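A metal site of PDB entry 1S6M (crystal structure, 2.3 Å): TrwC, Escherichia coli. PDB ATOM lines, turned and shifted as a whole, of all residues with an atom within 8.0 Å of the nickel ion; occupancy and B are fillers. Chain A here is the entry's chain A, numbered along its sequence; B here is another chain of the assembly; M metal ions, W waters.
O of Gln 159 sits at hydrogen-bond distance from ND1 of His 161 (2.8 Å). OG1 of Thr 87 is in hydrogen-bond range of ND1 of His 163 (3.3 Å). N of His 163 sits at hydrogen-bond distance from O of Phe 148, 2.8 Å away. ND1 of His 163 lies within hydrogen-bond range of OD2 of Asp 85 (3.5 Å). The backbone carbonyl oxygen of Tyr 18 sits at hydrogen-bond distance from a ring nitrogen (NE2) of His 150 (3.0 Å).
The nickel ion is bound by ND1 of His 150, NE2 of His 161, water W1, NE2 of His 163 and water W2. The nickel ion has five donor atoms within binding distance.
Of the 21 residues printed, 3 come within 4 Å of the nickel ion. The nearest printed residue that does not touch the nickel ion is Asp 21 (4.5 Å).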
ATOM      1  N   SER A  17      22.613 -13.705  22.514  1.00  0.00           N
ATOM      2  CA  SER A  17      21.493 -12.776  22.581  1.00  0.00           C
ATOM      3  C   SER A  17      20.614 -13.168  23.761  1.00  0.00           C
ATOM      4  O   SER A  17      19.530 -12.612  23.955  1.00  0.00           O
ATOM      5  CB  SER A  17      20.672 -12.837  21.289  1.00  0.00           C
ATOM      6  OG  SER A  17      19.402 -13.424  21.544  1.00  0.00           O
ATOM      7  N   TYR A  18      21.088 -14.135  24.547  1.00  0.00           N
ATOM      8  CA  TYR A  18      20.347 -14.565  25.714  1.00  0.00           C
ATOM      9  C   TYR A  18      20.408 -13.481  26.782  1.00  0.00           C
ATOM     10  O   TYR A  18      19.961 -13.688  27.902  1.00  0.00           O
ATOM     11  CB  TYR A  18      20.897 -15.900  26.245  1.00  0.00           C
ATOM     12  CG  TYR A  18      20.531 -17.093  25.396  1.00  0.00           C
ATOM     13  CD1 TYR A  18      19.329 -17.133  24.680  1.00  0.00           C
ATOM     14  CD2 TYR A  18      21.365 -18.204  25.316  1.00  0.00           C
ATOM     15  CE1 TYR A  18      18.977 -18.246  23.905  1.00  0.00           C
ATOM     16  CE2 TYR A  18      21.025 -19.324  24.542  1.00  0.00           C
ATOM     17  CZ  TYR A  18      19.831 -19.340  23.840  1.00  0.00           C
ATOM     18  OH  TYR A  18      19.472 -20.414  23.058  1.00  0.00           O
ATOM     19  N   ASP A  21      16.806 -10.852  25.527  1.00  0.00           N
ATOM     20  CA  ASP A  21      15.452 -11.392  25.737  1.00  0.00           C
ATOM     21  C   ASP A  21      14.888 -11.385  27.158  1.00  0.00           C
ATOM     22  O   ASP A  21      15.483 -10.829  28.085  1.00  0.00           O
ATOM     23  CB  ASP A  21      15.369 -12.837  25.229  1.00  0.00           C
ATOM     24  CG  ASP A  21      15.202 -12.918  23.721  1.00  0.00           C
ATOM     25  OD1 ASP A  21      15.041 -14.037  23.200  1.00  0.00           O
ATOM     26  OD2 ASP A  21      15.225 -11.851  23.063  1.00  0.00           O
ATOM     27  N   GLY A  22      13.728 -12.023  27.313  1.00  0.00           N
ATOM     28  CA  GLY A  22      13.099 -12.124  28.619  1.00  0.00           C
ATOM     29  C   GLY A  22      12.310 -10.920  29.076  1.00  0.00           C
ATOM     30  O   GLY A  22      11.462 -10.405  28.360  1.00  0.00           O
ATOM     31  N   ALA A  23      12.610 -10.486  30.295  1.00  0.00           N
ATOM     32  CA  ALA A  23      11.936  -9.338  30.878  1.00  0.00           C
ATOM     33  C   ALA A  23      12.755  -8.866  32.052  1.00  0.00           C
ATOM     34  O   ALA A  23      13.582  -9.607  32.591  1.00  0.00           O
ATOM     35  CB  ALA A  23      10.564  -9.739  31.336  1.00  0.00           C
ATOM     36  N   ASP A  85      22.040 -26.349  24.910  1.00  0.00           N
ATOM     37  CA  ASP A  85      21.074 -25.548  25.649  1.00  0.00           C
ATOM     38  C   ASP A  85      19.996 -26.413  26.307  1.00  0.00           C
ATOM     39  O   ASP A  85      19.314 -27.195  25.640  1.00  0.00           O
ATOM     40  CB  ASP A  85      20.400 -24.529  24.692  1.00  0.00           C
ATOM     41  CG  ASP A  85      19.435 -23.564  25.417  1.00  0.00           C
ATOM     42  OD1 ASP A  85      19.196 -23.732  26.637  1.00  0.00           O
ATOM     43  OD2 ASP A  85      18.920 -22.630  24.764  1.00  0.00           O
ATOM     44  N   THR A  87      16.698 -25.909  28.329  1.00  0.00           N
ATOM     45  CA  THR A  87      15.738 -24.887  28.713  1.00  0.00           C
ATOM     46  C   THR A  87      14.635 -25.356  29.669  1.00  0.00           C
ATOM     47  O   THR A  87      13.812 -26.199  29.300  1.00  0.00           O
ATOM     48  CB  THR A  87      15.080 -24.267  27.450  1.00  0.00           C
ATOM     49  OG1 THR A  87      16.086 -23.688  26.622  1.00  0.00           O
ATOM     50  CG2 THR A  87      14.080 -23.190  27.836  1.00  0.00           C
ATOM     51  N   SER A  89      11.244 -24.664  31.790  1.00  0.00           N
ATOM     52  CA  SER A  89      10.075 -23.789  31.790  1.00  0.00           C
ATOM     53  C   SER A  89       9.061 -24.161  32.882  1.00  0.00           C
ATOM     54  O   SER A  89       8.718 -25.323  33.060  1.00  0.00           O
ATOM     55  CB  SER A  89       9.375 -23.830  30.424  1.00  0.00           C
ATOM     56  OG  SER A  89      10.205 -23.290  29.411  1.00  0.00           O
ATOM     57  N   PHE A 148      20.760 -18.155  31.966  1.00  0.00           N
ATOM     58  CA  PHE A 148      20.037 -16.922  31.664  1.00  0.00           C
ATOM     59  C   PHE A 148      18.539 -17.065  31.923  1.00  0.00           C
ATOM     60  O   PHE A 148      17.873 -17.838  31.232  1.00  0.00           O
ATOM     61  CB  PHE A 148      20.281 -16.524  30.190  1.00  0.00           C
ATOM     62  CG  PHE A 148      21.737 -16.443  29.814  1.00  0.00           C
ATOM     63  CD1 PHE A 148      22.420 -17.566  29.348  1.00  0.00           C
ATOM     64  CD2 PHE A 148      22.448 -15.248  29.973  1.00  0.00           C
ATOM     65  CE1 PHE A 148      23.783 -17.502  29.033  1.00  0.00           C
ATOM     66  CE2 PHE A 148      23.807 -15.165  29.654  1.00  0.00           C
ATOM     67  CZ  PHE A 148      24.482 -16.299  29.191  1.00  0.00           C
ATOM     68  N   ARG A 149      18.030 -16.335  32.911  1.00  0.00           N
ATOM     69  CA  ARG A 149      16.604 -16.360  33.273  1.00  0.00           C
ATOM     70  C   ARG A 149      15.818 -15.299  32.479  1.00  0.00           C
ATOM     71  O   ARG A 149      16.227 -14.141  32.431  1.00  0.00           O
ATOM     72  CB  ARG A 149      16.447 -16.113  34.779  1.00  0.00           C
ATOM     73  CG  ARG A 149      15.046 -16.408  35.329  1.00  0.00           C
ATOM     74  CD  ARG A 149      14.974 -16.124  36.832  1.00  0.00           C
ATOM     75  NE  ARG A 149      15.160 -14.706  37.113  1.00  0.00           N
ATOM     76  CZ  ARG A 149      15.850 -14.224  38.141  1.00  0.00           C
ATOM     77  NH1 ARG A 149      15.961 -12.913  38.317  1.00  0.00           N
ATOM     78  NH2 ARG A 149      16.440 -15.051  39.001  1.00  0.00           N
ATOM     79  N   HIS A 150      14.692 -15.705  31.886  1.00  0.00           N
ATOM     80  CA  HIS A 150      13.827 -14.848  31.080  1.00  0.00           C
ATOM     81  C   HIS A 150      12.404 -14.807  31.673  1.00  0.00           C
ATOM     82  O   HIS A 150      12.044 -15.659  32.483  1.00  0.00           O
ATOM     83  CB  HIS A 150      13.789 -15.363  29.614  1.00  0.00           C
ATOM     84  CG  HIS A 150      15.083 -15.158  28.874  1.00  0.00           C
ATOM     85  ND1 HIS A 150      15.306 -15.647  27.600  1.00  0.00           N
ATOM     86  CD2 HIS A 150      16.189 -14.498  29.302  1.00  0.00           C
ATOM     87  CE1 HIS A 150      16.552 -15.266  27.267  1.00  0.00           C
ATOM     88  NE2 HIS A 150      17.103 -14.578  28.271  1.00  0.00           N
ATOM     89  N   GLU A 151      11.602 -13.828  31.267  1.00  0.00           N
ATOM     90  CA  GLU A 151      10.251 -13.698  31.816  1.00  0.00           C
ATOM     91  C   GLU A 151       9.065 -13.643  30.833  1.00  0.00           C
ATOM     92  O   GLU A 151       7.927 -13.692  31.272  1.00  0.00           O
ATOM     93  CB  GLU A 151      10.183 -12.478  32.751  1.00  0.00           C
ATOM     94  CG  GLU A 151      11.187 -12.503  33.905  1.00  0.00           C
ATOM     95  CD  GLU A 151      11.089 -11.259  34.786  1.00  0.00           C
ATOM     96  OE1 GLU A 151      10.323 -10.333  34.440  1.00  0.00           O
ATOM     97  OE2 GLU A 151      11.772 -11.201  35.832  1.00  0.00           O
ATOM     98  N   THR A 152       9.319 -13.552  29.525  1.00  0.00           N
ATOM     99  CA  THR A 152       8.210 -13.458  28.559  1.00  0.00           C
ATOM    100  C   THR A 152       8.272 -14.437  27.378  1.00  0.00           C
ATOM    101  O   THR A 152       9.341 -14.898  27.001  1.00  0.00           O
ATOM    102  CB  THR A 152       8.116 -12.029  27.956  1.00  0.00           C
ATOM    103  OG1 THR A 152       9.283 -11.762  27.182  1.00  0.00           O
ATOM    104  CG2 THR A 152       8.003 -10.983  29.054  1.00  0.00           C
ATOM    105  N   SER A 153       7.110 -14.744  26.798  1.00  0.00           N
ATOM    106  CA  SER A 153       7.036 -15.631  25.638  1.00  0.00           C
ATOM    107  C   SER A 153       7.120 -14.766  24.373  1.00  0.00           C
ATOM    108  O   SER A 153       7.165 -13.535  24.469  1.00  0.00           O
ATOM    109  CB  SER A 153       5.719 -16.416  25.620  1.00  0.00           C
ATOM    110  OG  SER A 153       4.648 -15.622  25.169  1.00  0.00           O
ATOM    111  N   ARG A 154       7.132 -15.389  23.203  1.00  0.00           N
ATOM    112  CA  ARG A 154       7.228 -14.645  21.943  1.00  0.00           C
ATOM    113  C   ARG A 154       6.008 -13.728  21.733  1.00  0.00           C
ATOM    114  O   ARG A 154       6.098 -12.735  21.004  1.00  0.00           O
ATOM    115  CB  ARG A 154       7.389 -15.605  20.762  1.00  0.00           C
ATOM    116  CG  ARG A 154       7.444 -14.947  19.369  1.00  0.00           C
ATOM    117  CD  ARG A 154       8.700 -14.075  19.147  1.00  0.00           C
ATOM    118  NE  ARG A 154       9.957 -14.828  19.208  1.00  0.00           N
ATOM    119  CZ  ARG A 154      10.626 -15.281  18.160  1.00  0.00           C
ATOM    120  NH1 ARG A 154      11.769 -15.950  18.333  1.00  0.00           N
ATOM    121  NH2 ARG A 154      10.175 -15.084  16.921  1.00  0.00           N
ATOM    122  N   GLN A 159       6.037 -15.841  31.152  1.00  0.00           N
ATOM    123  CA  GLN A 159       6.597 -17.165  30.839  1.00  0.00           C
ATOM    124  C   GLN A 159       7.975 -17.351  31.499  1.00  0.00           C
ATOM    125  O   GLN A 159       9.016 -17.151  30.871  1.00  0.00           O
ATOM    126  CB  GLN A 159       6.693 -17.303  29.315  1.00  0.00           C
ATOM    127  CG  GLN A 159       7.248 -18.621  28.776  1.00  0.00           C
ATOM    128  CD  GLN A 159       6.402 -19.833  29.132  1.00  0.00           C
ATOM    129  OE1 GLN A 159       5.251 -19.703  29.545  1.00  0.00           O
ATOM    130  NE2 GLN A 159       6.975 -21.022  28.964  1.00  0.00           N
ATOM    131  N   LEU A 160       7.970 -17.722  32.776  1.00  0.00           N
ATOM    132  CA  LEU A 160       9.205 -17.918  33.520  1.00  0.00           C
ATOM    133  C   LEU A 160      10.025 -19.095  33.014  1.00  0.00           C
ATOM    134  O   LEU A 160       9.568 -20.228  33.029  1.00  0.00           O
ATOM    135  CB  LEU A 160       8.890 -18.130  35.011  1.00  0.00           C
ATOM    136  CG  LEU A 160      10.047 -18.252  36.000  1.00  0.00           C
ATOM    137  CD1 LEU A 160      10.926 -16.997  35.929  1.00  0.00           C
ATOM    138  CD2 LEU A 160       9.492 -18.420  37.417  1.00  0.00           C
ATOM    139  N   HIS A 161      11.245 -18.818  32.552  1.00  0.00           N
ATOM    140  CA  HIS A 161      12.109 -19.878  32.070  1.00  0.00           C
ATOM    141  C   HIS A 161      13.587 -19.513  32.165  1.00  0.00           C
ATOM    142  O   HIS A 161      13.932 -18.339  32.312  1.00  0.00           O
ATOM    143  CB  HIS A 161      11.774 -20.263  30.607  1.00  0.00           C
ATOM    144  CG  HIS A 161      12.001 -19.173  29.602  1.00  0.00           C
ATOM    145  ND1 HIS A 161      11.096 -18.151  29.358  1.00  0.00           N
ATOM    146  CD2 HIS A 161      13.021 -19.008  28.717  1.00  0.00           C
ATOM    147  CE1 HIS A 161      11.576 -17.406  28.357  1.00  0.00           C
ATOM    148  NE2 HIS A 161      12.719 -17.900  27.951  1.00  0.00           N
ATOM    149  N   THR A 162      14.439 -20.532  32.115  1.00  0.00           N
ATOM    150  CA  THR A 162      15.881 -20.336  32.177  1.00  0.00           C
ATOM    151  C   THR A 162      16.593 -21.167  31.114  1.00  0.00           C
ATOM    152  O   THR A 162      16.341 -22.357  30.953  1.00  0.00           O
ATOM    153  CB  THR A 162      16.485 -20.749  33.543  1.00  0.00           C
ATOM    154  OG1 THR A 162      15.972 -19.903  34.589  1.00  0.00           O
ATOM    155  CG2 THR A 162      17.990 -20.621  33.513  1.00  0.00           C
ATOM    156  N   HIS A 163      17.483 -20.511  30.370  1.00  0.00           N
ATOM    157  CA  HIS A 163      18.281 -21.160  29.354  1.00  0.00           C
ATOM    158  C   HIS A 163      19.609 -21.532  30.016  1.00  0.00           C
ATOM    159  O   HIS A 163      20.410 -20.650  30.336  1.00  0.00           O
ATOM    160  CB  HIS A 163      18.587 -20.212  28.190  1.00  0.00           C
ATOM    161  CG  HIS A 163      17.368 -19.753  27.441  1.00  0.00           C
ATOM    162  ND1 HIS A 163      16.754 -20.482  26.450  1.00  0.00           N
ATOM    163  CD2 HIS A 163      16.679 -18.578  27.549  1.00  0.00           C
ATOM    164  CE1 HIS A 163      15.735 -19.765  25.981  1.00  0.00           C
ATOM    165  NE2 HIS A 163      15.667 -18.615  26.613  1.00  0.00           N
ATOM    166  P    DT B  25       7.845 -20.504  21.407  1.00  0.00           P
ATOM    167  OP1  DT B  25       7.047 -19.319  20.987  1.00  0.00           O
ATOM    168  OP2  DT B  25       7.743 -21.753  20.643  1.00  0.00           O
ATOM    169  O5'  DT B  25       9.396 -20.112  21.460  1.00  0.00           O
ATOM    170  C5'  DT B  25      10.308 -20.765  22.364  1.00  0.00           C
ATOM    171  C4'  DT B  25      11.760 -20.569  21.944  1.00  0.00           C
ATOM    172  O4'  DT B  25      12.350 -21.802  21.486  1.00  0.00           O
ATOM    173  C3'  DT B  25      11.930 -19.620  20.758  1.00  0.00           C
ATOM    174  O3'  DT B  25      12.076 -18.294  21.287  1.00  0.00           O
ATOM    175  C2'  DT B  25      13.222 -20.075  20.087  1.00  0.00           C
ATOM    176  C1'  DT B  25      13.340 -21.527  20.498  1.00  0.00           C
ATOM    177  N1   DT B  25      13.275 -22.576  19.454  1.00  0.00           N
ATOM    178  C2   DT B  25      12.146 -23.343  19.399  1.00  0.00           C
ATOM    179  O2   DT B  25      11.167 -23.143  20.101  1.00  0.00           O
ATOM    180  N3   DT B  25      12.207 -24.379  18.507  1.00  0.00           N
ATOM    181  C4   DT B  25      13.251 -24.689  17.659  1.00  0.00           C
ATOM    182  O4   DT B  25      13.167 -25.669  16.929  1.00  0.00           O
ATOM    183  C5   DT B  25      14.380 -23.797  17.718  1.00  0.00           C
ATOM    184  C7   DT B  25      15.545 -24.026  16.793  1.00  0.00           C
ATOM    185  C6   DT B  25      14.333 -22.792  18.595  1.00  0.00           C
HETATM  186 NI    NI M   1      14.076 -17.014  26.500  1.00  0.00          NI
HETATM  187  O   HOH W   1      12.993 -18.180  24.907  1.00  0.00           O
HETATM  188  O   HOH W   2      15.279 -16.353  24.687  1.00  0.00           O
